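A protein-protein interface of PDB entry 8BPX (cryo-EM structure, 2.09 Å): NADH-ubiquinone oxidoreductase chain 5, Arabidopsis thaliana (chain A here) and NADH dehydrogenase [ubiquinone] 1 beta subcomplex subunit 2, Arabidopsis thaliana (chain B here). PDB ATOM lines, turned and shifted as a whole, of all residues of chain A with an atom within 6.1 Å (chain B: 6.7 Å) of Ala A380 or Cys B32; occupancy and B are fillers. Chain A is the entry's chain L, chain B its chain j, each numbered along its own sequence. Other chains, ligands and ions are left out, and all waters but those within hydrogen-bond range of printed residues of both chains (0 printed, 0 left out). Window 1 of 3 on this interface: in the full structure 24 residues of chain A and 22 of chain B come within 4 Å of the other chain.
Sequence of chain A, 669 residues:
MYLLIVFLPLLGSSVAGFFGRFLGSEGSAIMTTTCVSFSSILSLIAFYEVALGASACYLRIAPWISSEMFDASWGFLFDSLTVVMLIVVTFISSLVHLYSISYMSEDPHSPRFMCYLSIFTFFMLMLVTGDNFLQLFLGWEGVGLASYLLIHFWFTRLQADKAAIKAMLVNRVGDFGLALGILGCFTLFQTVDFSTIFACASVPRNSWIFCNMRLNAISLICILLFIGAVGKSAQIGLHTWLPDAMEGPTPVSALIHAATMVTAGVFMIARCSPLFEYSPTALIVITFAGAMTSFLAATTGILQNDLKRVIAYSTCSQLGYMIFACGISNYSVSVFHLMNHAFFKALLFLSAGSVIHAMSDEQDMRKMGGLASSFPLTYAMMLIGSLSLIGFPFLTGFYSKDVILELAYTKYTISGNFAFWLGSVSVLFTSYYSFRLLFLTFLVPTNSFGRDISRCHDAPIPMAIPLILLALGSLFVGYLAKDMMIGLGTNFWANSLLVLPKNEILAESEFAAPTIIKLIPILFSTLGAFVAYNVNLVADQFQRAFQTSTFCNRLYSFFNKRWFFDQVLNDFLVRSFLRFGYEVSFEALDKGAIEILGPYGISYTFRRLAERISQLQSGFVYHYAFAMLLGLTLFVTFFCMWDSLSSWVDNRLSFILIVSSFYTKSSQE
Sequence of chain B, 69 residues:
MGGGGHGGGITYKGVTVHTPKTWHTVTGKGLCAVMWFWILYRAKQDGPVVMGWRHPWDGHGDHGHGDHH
Along chain B the printed residues that touch a printed residue of chain A span positions 27 to 35.
Hydrophobic or aromatic side chains of chain A within 4 Å of the printed part of chain B: Leu A377, Ala A380, Met A381, Leu A383 and Ile A384.
Along chain A the printed residues that touch a printed residue of chain B span positions 377 to 384.
Among the printed residues, 6 pairs touch across the chains.
Among the printed residues, no Asp or Glu carboxylate lies within 4 Å of a Lys or Arg side-chain nitrogen of the other chain.
Ala A380 touches just these residues of chain B: Gly B28 and Cys B32.
Cys B32 touches two residues of chain A.
Of the printed residues of chain A, Thr B27 touches Leu A377.
Of the printed residues of chain B, Leu A383 touches Cys B32.
Of the printed residues of chain A, Leu B31 touches Met A381.
Printed residues of chain B within 4 Å of Met A381: Leu B31 (3.9 Å).
Of the printed residues of chain A, Met B35 touches Ile A384 (3.6 Å).
Gly A385 touches none of the printed residues of chain B.
The nearest residue of chain B that does not touch Ala A380 is Lys B29 (5.3 Å).
The nearest printed residue of chain A that does not touch Met B35 is Leu A383 (4.3 Å).
Leu A377 touches Thr B27.
CA of Gly B28 touches CB of Ala A380 (3.8 Å).
Ala A380 touches Cys B32 (CB to SG, 3.7 Å).
Met A381 touches Leu B31.
CD2 of Leu A383 touches SG of Cys B32, 3.9 Å away.
Ile A384 touches Met B35 (CG1 to SD, 3.6 Å).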
ATOM      1  N   PHE A 375     -15.708  29.152  29.770  1.00  0.00           N
ATOM      2  CA  PHE A 375     -14.591  28.233  29.569  1.00  0.00           C
ATOM      3  C   PHE A 375     -15.139  26.814  29.518  1.00  0.00           C
ATOM      4  O   PHE A 375     -15.015  26.052  30.487  1.00  0.00           O
ATOM      5  CB  PHE A 375     -13.530  28.369  30.661  1.00  0.00           C
ATOM      6  CG  PHE A 375     -13.233  29.782  31.049  1.00  0.00           C
ATOM      7  CD1 PHE A 375     -13.342  30.192  32.363  1.00  0.00           C
ATOM      8  CD2 PHE A 375     -12.836  30.704  30.097  1.00  0.00           C
ATOM      9  CE1 PHE A 375     -13.055  31.494  32.721  1.00  0.00           C
ATOM     10  CE2 PHE A 375     -12.560  32.002  30.447  1.00  0.00           C
ATOM     11  CZ  PHE A 375     -12.669  32.399  31.761  1.00  0.00           C
ATOM     12  N   PRO A 376     -15.744  26.419  28.394  1.00  0.00           N
ATOM     13  CA  PRO A 376     -16.346  25.076  28.330  1.00  0.00           C
ATOM     14  C   PRO A 376     -15.326  23.960  28.441  1.00  0.00           C
ATOM     15  O   PRO A 376     -15.517  23.018  29.219  1.00  0.00           O
ATOM     16  CB  PRO A 376     -17.046  25.075  26.960  1.00  0.00           C
ATOM     17  CG  PRO A 376     -17.055  26.493  26.509  1.00  0.00           C
ATOM     18  CD  PRO A 376     -15.872  27.143  27.124  1.00  0.00           C
ATOM     19  N   LEU A 377     -14.239  24.045  27.670  1.00  0.00           N
ATOM     20  CA  LEU A 377     -13.237  22.988  27.672  1.00  0.00           C
ATOM     21  C   LEU A 377     -12.583  22.841  29.039  1.00  0.00           C
ATOM     22  O   LEU A 377     -12.405  21.722  29.538  1.00  0.00           O
ATOM     23  CB  LEU A 377     -12.185  23.272  26.603  1.00  0.00           C
ATOM     24  CG  LEU A 377     -10.971  22.342  26.609  1.00  0.00           C
ATOM     25  CD1 LEU A 377     -11.409  20.909  26.372  1.00  0.00           C
ATOM     26  CD2 LEU A 377      -9.950  22.784  25.577  1.00  0.00           C
ATOM     27  N   THR A 378     -12.225  23.962  29.662  1.00  0.00           N
ATOM     28  CA  THR A 378     -11.584  23.899  30.968  1.00  0.00           C
ATOM     29  C   THR A 378     -12.540  23.354  32.024  1.00  0.00           C
ATOM     30  O   THR A 378     -12.143  22.536  32.863  1.00  0.00           O
ATOM     31  CB  THR A 378     -11.061  25.281  31.358  1.00  0.00           C
ATOM     32  OG1 THR A 378      -9.883  25.575  30.600  1.00  0.00           O
ATOM     33  CG2 THR A 378     -10.702  25.298  32.808  1.00  0.00           C
ATOM     34  N   TYR A 379     -13.779  23.832  32.038  1.00  0.00           N
ATOM     35  CA  TYR A 379     -14.814  23.256  32.925  1.00  0.00           C
ATOM     36  C   TYR A 379     -14.948  21.718  32.722  1.00  0.00           C
ATOM     37  O   TYR A 379     -15.003  21.023  33.709  1.00  0.00           O
ATOM     38  CB  TYR A 379     -16.197  23.887  32.755  1.00  0.00           C
ATOM     39  CG  TYR A 379     -17.260  23.163  33.541  1.00  0.00           C
ATOM     40  CD1 TYR A 379     -17.208  23.131  34.924  1.00  0.00           C
ATOM     41  CD2 TYR A 379     -18.271  22.456  32.919  1.00  0.00           C
ATOM     42  CE1 TYR A 379     -18.146  22.450  35.672  1.00  0.00           C
ATOM     43  CE2 TYR A 379     -19.223  21.769  33.650  1.00  0.00           C
ATOM     44  CZ  TYR A 379     -19.160  21.769  35.029  1.00  0.00           C
ATOM     45  OH  TYR A 379     -20.077  21.092  35.764  1.00  0.00           O
ATOM     46  N   ALA A 380     -14.998  21.262  31.484  1.00  0.00           N
ATOM     47  CA  ALA A 380     -15.128  19.828  31.239  1.00  0.00           C
ATOM     48  C   ALA A 380     -13.920  19.066  31.767  1.00  0.00           C
ATOM     49  O   ALA A 380     -14.065  17.988  32.357  1.00  0.00           O
ATOM     50  CB  ALA A 380     -15.324  19.559  29.749  1.00  0.00           C
ATOM     51  N   MET A 381     -12.716  19.611  31.566  1.00  0.00           N
ATOM     52  CA  MET A 381     -11.517  18.966  32.091  1.00  0.00           C
ATOM     53  C   MET A 381     -11.555  18.887  33.610  1.00  0.00           C
ATOM     54  O   MET A 381     -11.234  17.844  34.196  1.00  0.00           O
ATOM     55  CB  MET A 381     -10.266  19.712  31.629  1.00  0.00           C
ATOM     56  CG  MET A 381      -9.989  19.738  30.123  1.00  0.00           C
ATOM     57  SD  MET A 381      -9.837  18.173  29.227  1.00  0.00           S
ATOM     58  CE  MET A 381     -11.541  17.696  28.940  1.00  0.00           C
ATOM     59  N   MET A 382     -11.959  19.976  34.264  1.00  0.00           N
ATOM     60  CA  MET A 382     -12.044  19.970  35.719  1.00  0.00           C
ATOM     61  C   MET A 382     -13.100  18.986  36.205  1.00  0.00           C
ATOM     62  O   MET A 382     -12.900  18.300  37.211  1.00  0.00           O
ATOM     63  CB  MET A 382     -12.326  21.379  36.239  1.00  0.00           C
ATOM     64  CG  MET A 382     -11.976  21.571  37.708  1.00  0.00           C
ATOM     65  SD  MET A 382     -10.412  22.427  37.985  1.00  0.00           S
ATOM     66  CE  MET A 382     -10.690  23.938  37.079  1.00  0.00           C
ATOM     67  N   LEU A 383     -14.234  18.894  35.536  1.00  0.00           N
ATOM     68  CA  LEU A 383     -15.298  17.901  35.858  1.00  0.00           C
ATOM     69  C   LEU A 383     -14.752  16.473  35.783  1.00  0.00           C
ATOM     70  O   LEU A 383     -14.875  15.764  36.730  1.00  0.00           O
ATOM     71  CB  LEU A 383     -16.475  18.078  34.909  1.00  0.00           C
ATOM     72  CG  LEU A 383     -17.646  17.121  35.099  1.00  0.00           C
ATOM     73  CD1 LEU A 383     -18.261  17.274  36.475  1.00  0.00           C
ATOM     74  CD2 LEU A 383     -18.686  17.329  34.013  1.00  0.00           C
ATOM     75  N   ILE A 384     -14.101  16.183  34.672  1.00  0.00           N
ATOM     76  CA  ILE A 384     -13.593  14.825  34.490  1.00  0.00           C
ATOM     77  C   ILE A 384     -12.570  14.494  35.571  1.00  0.00           C
ATOM     78  O   ILE A 384     -12.614  13.420  36.185  1.00  0.00           O
ATOM     79  CB  ILE A 384     -13.004  14.661  33.077  1.00  0.00           C
ATOM     80  CG1 ILE A 384     -14.122  14.594  32.034  1.00  0.00           C
ATOM     81  CG2 ILE A 384     -12.099  13.439  32.999  1.00  0.00           C
ATOM     82  CD1 ILE A 384     -13.641  14.677  30.618  1.00  0.00           C
ATOM     83  N   GLY A 385     -11.646  15.422  35.831  1.00  0.00           N
ATOM     84  CA  GLY A 385     -10.663  15.195  36.875  1.00  0.00           C
ATOM     85  C   GLY A 385     -11.290  15.013  38.241  1.00  0.00           C
ATOM     86  O   GLY A 385     -10.900  14.125  38.999  1.00  0.00           O
ATOM     87  N   THR B  27     -15.026  20.176  21.767  1.00  0.00           N
ATOM     88  CA  THR B  27     -14.167  19.222  22.457  1.00  0.00           C
ATOM     89  C   THR B  27     -14.681  18.926  23.861  1.00  0.00           C
ATOM     90  O   THR B  27     -14.703  17.764  24.288  1.00  0.00           O
ATOM     91  CB  THR B  27     -12.736  19.757  22.499  1.00  0.00           C
ATOM     92  OG1 THR B  27     -12.216  19.836  21.167  1.00  0.00           O
ATOM     93  CG2 THR B  27     -11.847  18.856  23.318  1.00  0.00           C
ATOM     94  N   GLY B  28     -15.106  19.960  24.595  1.00  0.00           N
ATOM     95  CA  GLY B  28     -15.661  19.720  25.920  1.00  0.00           C
ATOM     96  C   GLY B  28     -16.927  18.887  25.876  1.00  0.00           C
ATOM     97  O   GLY B  28     -17.060  17.888  26.597  1.00  0.00           O
ATOM     98  N   LYS B  29     -17.936  19.337  25.101  1.00  0.00           N
ATOM     99  CA  LYS B  29     -19.124  18.465  24.907  1.00  0.00           C
ATOM    100  C   LYS B  29     -18.701  17.024  24.558  1.00  0.00           C
ATOM    101  O   LYS B  29     -19.089  16.197  25.346  1.00  0.00           O
ATOM    102  CB  LYS B  29     -20.130  19.039  23.904  1.00  0.00           C
ATOM    103  CG  LYS B  29     -20.982  20.189  24.409  1.00  0.00           C
ATOM    104  CD  LYS B  29     -22.254  19.722  25.062  1.00  0.00           C
ATOM    105  CE  LYS B  29     -23.065  20.837  25.686  1.00  0.00           C
ATOM    106  NZ  LYS B  29     -22.273  21.599  26.678  1.00  0.00           N
ATOM    107  N   GLY B  30     -17.849  16.779  23.552  1.00  0.00           N
ATOM    108  CA  GLY B  30     -17.604  15.421  23.108  1.00  0.00           C
ATOM    109  C   GLY B  30     -16.882  14.567  24.125  1.00  0.00           C
ATOM    110  O   GLY B  30     -17.222  13.397  24.307  1.00  0.00           O
ATOM    111  N   LEU B  31     -15.866  15.122  24.791  1.00  0.00           N
ATOM    112  CA  LEU B  31     -15.183  14.349  25.820  1.00  0.00           C
ATOM    113  C   LEU B  31     -16.120  14.007  26.967  1.00  0.00           C
ATOM    114  O   LEU B  31     -16.110  12.872  27.460  1.00  0.00           O
ATOM    115  CB  LEU B  31     -13.948  15.085  26.331  1.00  0.00           C
ATOM    116  CG  LEU B  31     -12.682  14.826  25.523  1.00  0.00           C
ATOM    117  CD1 LEU B  31     -11.830  16.064  25.442  1.00  0.00           C
ATOM    118  CD2 LEU B  31     -11.900  13.689  26.151  1.00  0.00           C
ATOM    119  N   CYS B  32     -16.925  14.948  27.420  1.00  0.00           N
ATOM    120  CA  CYS B  32     -17.888  14.561  28.457  1.00  0.00           C
ATOM    121  C   CYS B  32     -18.895  13.519  27.928  1.00  0.00           C
ATOM    122  O   CYS B  32     -19.245  12.658  28.720  1.00  0.00           O
ATOM    123  CB  CYS B  32     -18.536  15.793  29.100  1.00  0.00           C
ATOM    124  SG  CYS B  32     -17.461  16.573  30.337  1.00  0.00           S
ATOM    125  N   ALA B  33     -19.284  13.573  26.661  1.00  0.00           N
ATOM    126  CA  ALA B  33     -20.305  12.633  26.119  1.00  0.00           C
ATOM    127  C   ALA B  33     -19.672  11.258  26.120  1.00  0.00           C
ATOM    128  O   ALA B  33     -20.309  10.332  26.644  1.00  0.00           O
ATOM    129  CB  ALA B  33     -20.801  13.070  24.755  1.00  0.00           C
ATOM    130  N   VAL B  34     -18.398  11.232  25.762  1.00  0.00           N
ATOM    131  CA  VAL B  34     -17.658   9.977  25.777  1.00  0.00           C
ATOM    132  C   VAL B  34     -17.587   9.426  27.191  1.00  0.00           C
ATOM    133  O   VAL B  34     -17.754   8.223  27.412  1.00  0.00           O
ATOM    134  CB  VAL B  34     -16.253  10.180  25.173  1.00  0.00           C
ATOM    135  CG1 VAL B  34     -15.272   9.155  25.710  1.00  0.00           C
ATOM    136  CG2 VAL B  34     -16.309  10.107  23.666  1.00  0.00           C
ATOM    137  N   MET B  35     -17.351  10.300  28.176  1.00  0.00           N
ATOM    138  CA  MET B  35     -17.297   9.856  29.566  1.00  0.00           C
ATOM    139  C   MET B  35     -18.636   9.281  30.025  1.00  0.00           C
ATOM    140  O   MET B  35     -18.679   8.227  30.672  1.00  0.00           O
ATOM    141  CB  MET B  35     -16.874  11.019  30.463  1.00  0.00           C
ATOM    142  CG  MET B  35     -17.202  10.838  31.934  1.00  0.00           C
ATOM    143  SD  MET B  35     -16.768  12.274  32.936  1.00  0.00           S
ATOM    144  CE  MET B  35     -17.960  13.474  32.342  1.00  0.00           C
ATOM    145  N   TRP B  36     -19.737   9.925  29.729  1.00  0.00           N
ATOM    146  CA  TRP B  36     -21.112   9.467  30.103  1.00  0.00           C
ATOM    147  C   TRP B  36     -21.427   8.130  29.420  1.00  0.00           C
ATOM    148  O   TRP B  36     -21.890   7.235  30.118  1.00  0.00           O
ATOM    149  CB  TRP B  36     -22.176  10.529  29.816  1.00  0.00           C
ATOM    150  CG  TRP B  36     -21.975  11.853  30.482  1.00  0.00           C
ATOM    151  CD1 TRP B  36     -21.884  13.069  29.874  1.00  0.00           C
ATOM    152  CD2 TRP B  36     -21.852  12.103  31.892  1.00  0.00           C
ATOM    153  NE1 TRP B  36     -21.701  14.054  30.798  1.00  0.00           N
ATOM    154  CE2 TRP B  36     -21.682  13.495  32.047  1.00  0.00           C
ATOM    155  CE3 TRP B  36     -21.865  11.300  33.032  1.00  0.00           C
ATOM    156  CZ2 TRP B  36     -21.540  14.088  33.300  1.00  0.00           C
ATOM    157  CZ3 TRP B  36     -21.709  11.881  34.269  1.00  0.00           C
ATOM    158  CH2 TRP B  36     -21.551  13.264  34.399  1.00  0.00           C
ATOM    159  N   PHE B  37     -21.080   8.009  28.150  1.00  0.00           N
ATOM    160  CA  PHE B  37     -21.305   6.748  27.453  1.00  0.00           C
ATOM    161  C   PHE B  37     -20.455   5.634  28.044  1.00  0.00           C
ATOM    162  O   PHE B  37     -20.923   4.502  28.199  1.00  0.00           O
ATOM    163  CB  PHE B  37     -21.005   6.901  25.962  1.00  0.00           C
ATOM    164  CG  PHE B  37     -21.157   5.624  25.179  1.00  0.00           C
ATOM    165  CD1 PHE B  37     -20.078   4.780  24.976  1.00  0.00           C
ATOM    166  CD2 PHE B  37     -22.387   5.266  24.646  1.00  0.00           C
ATOM    167  CE1 PHE B  37     -20.217   3.610  24.264  1.00  0.00           C
ATOM    168  CE2 PHE B  37     -22.530   4.099  23.931  1.00  0.00           C
ATOM    169  CZ  PHE B  37     -21.444   3.269  23.737  1.00  0.00           C
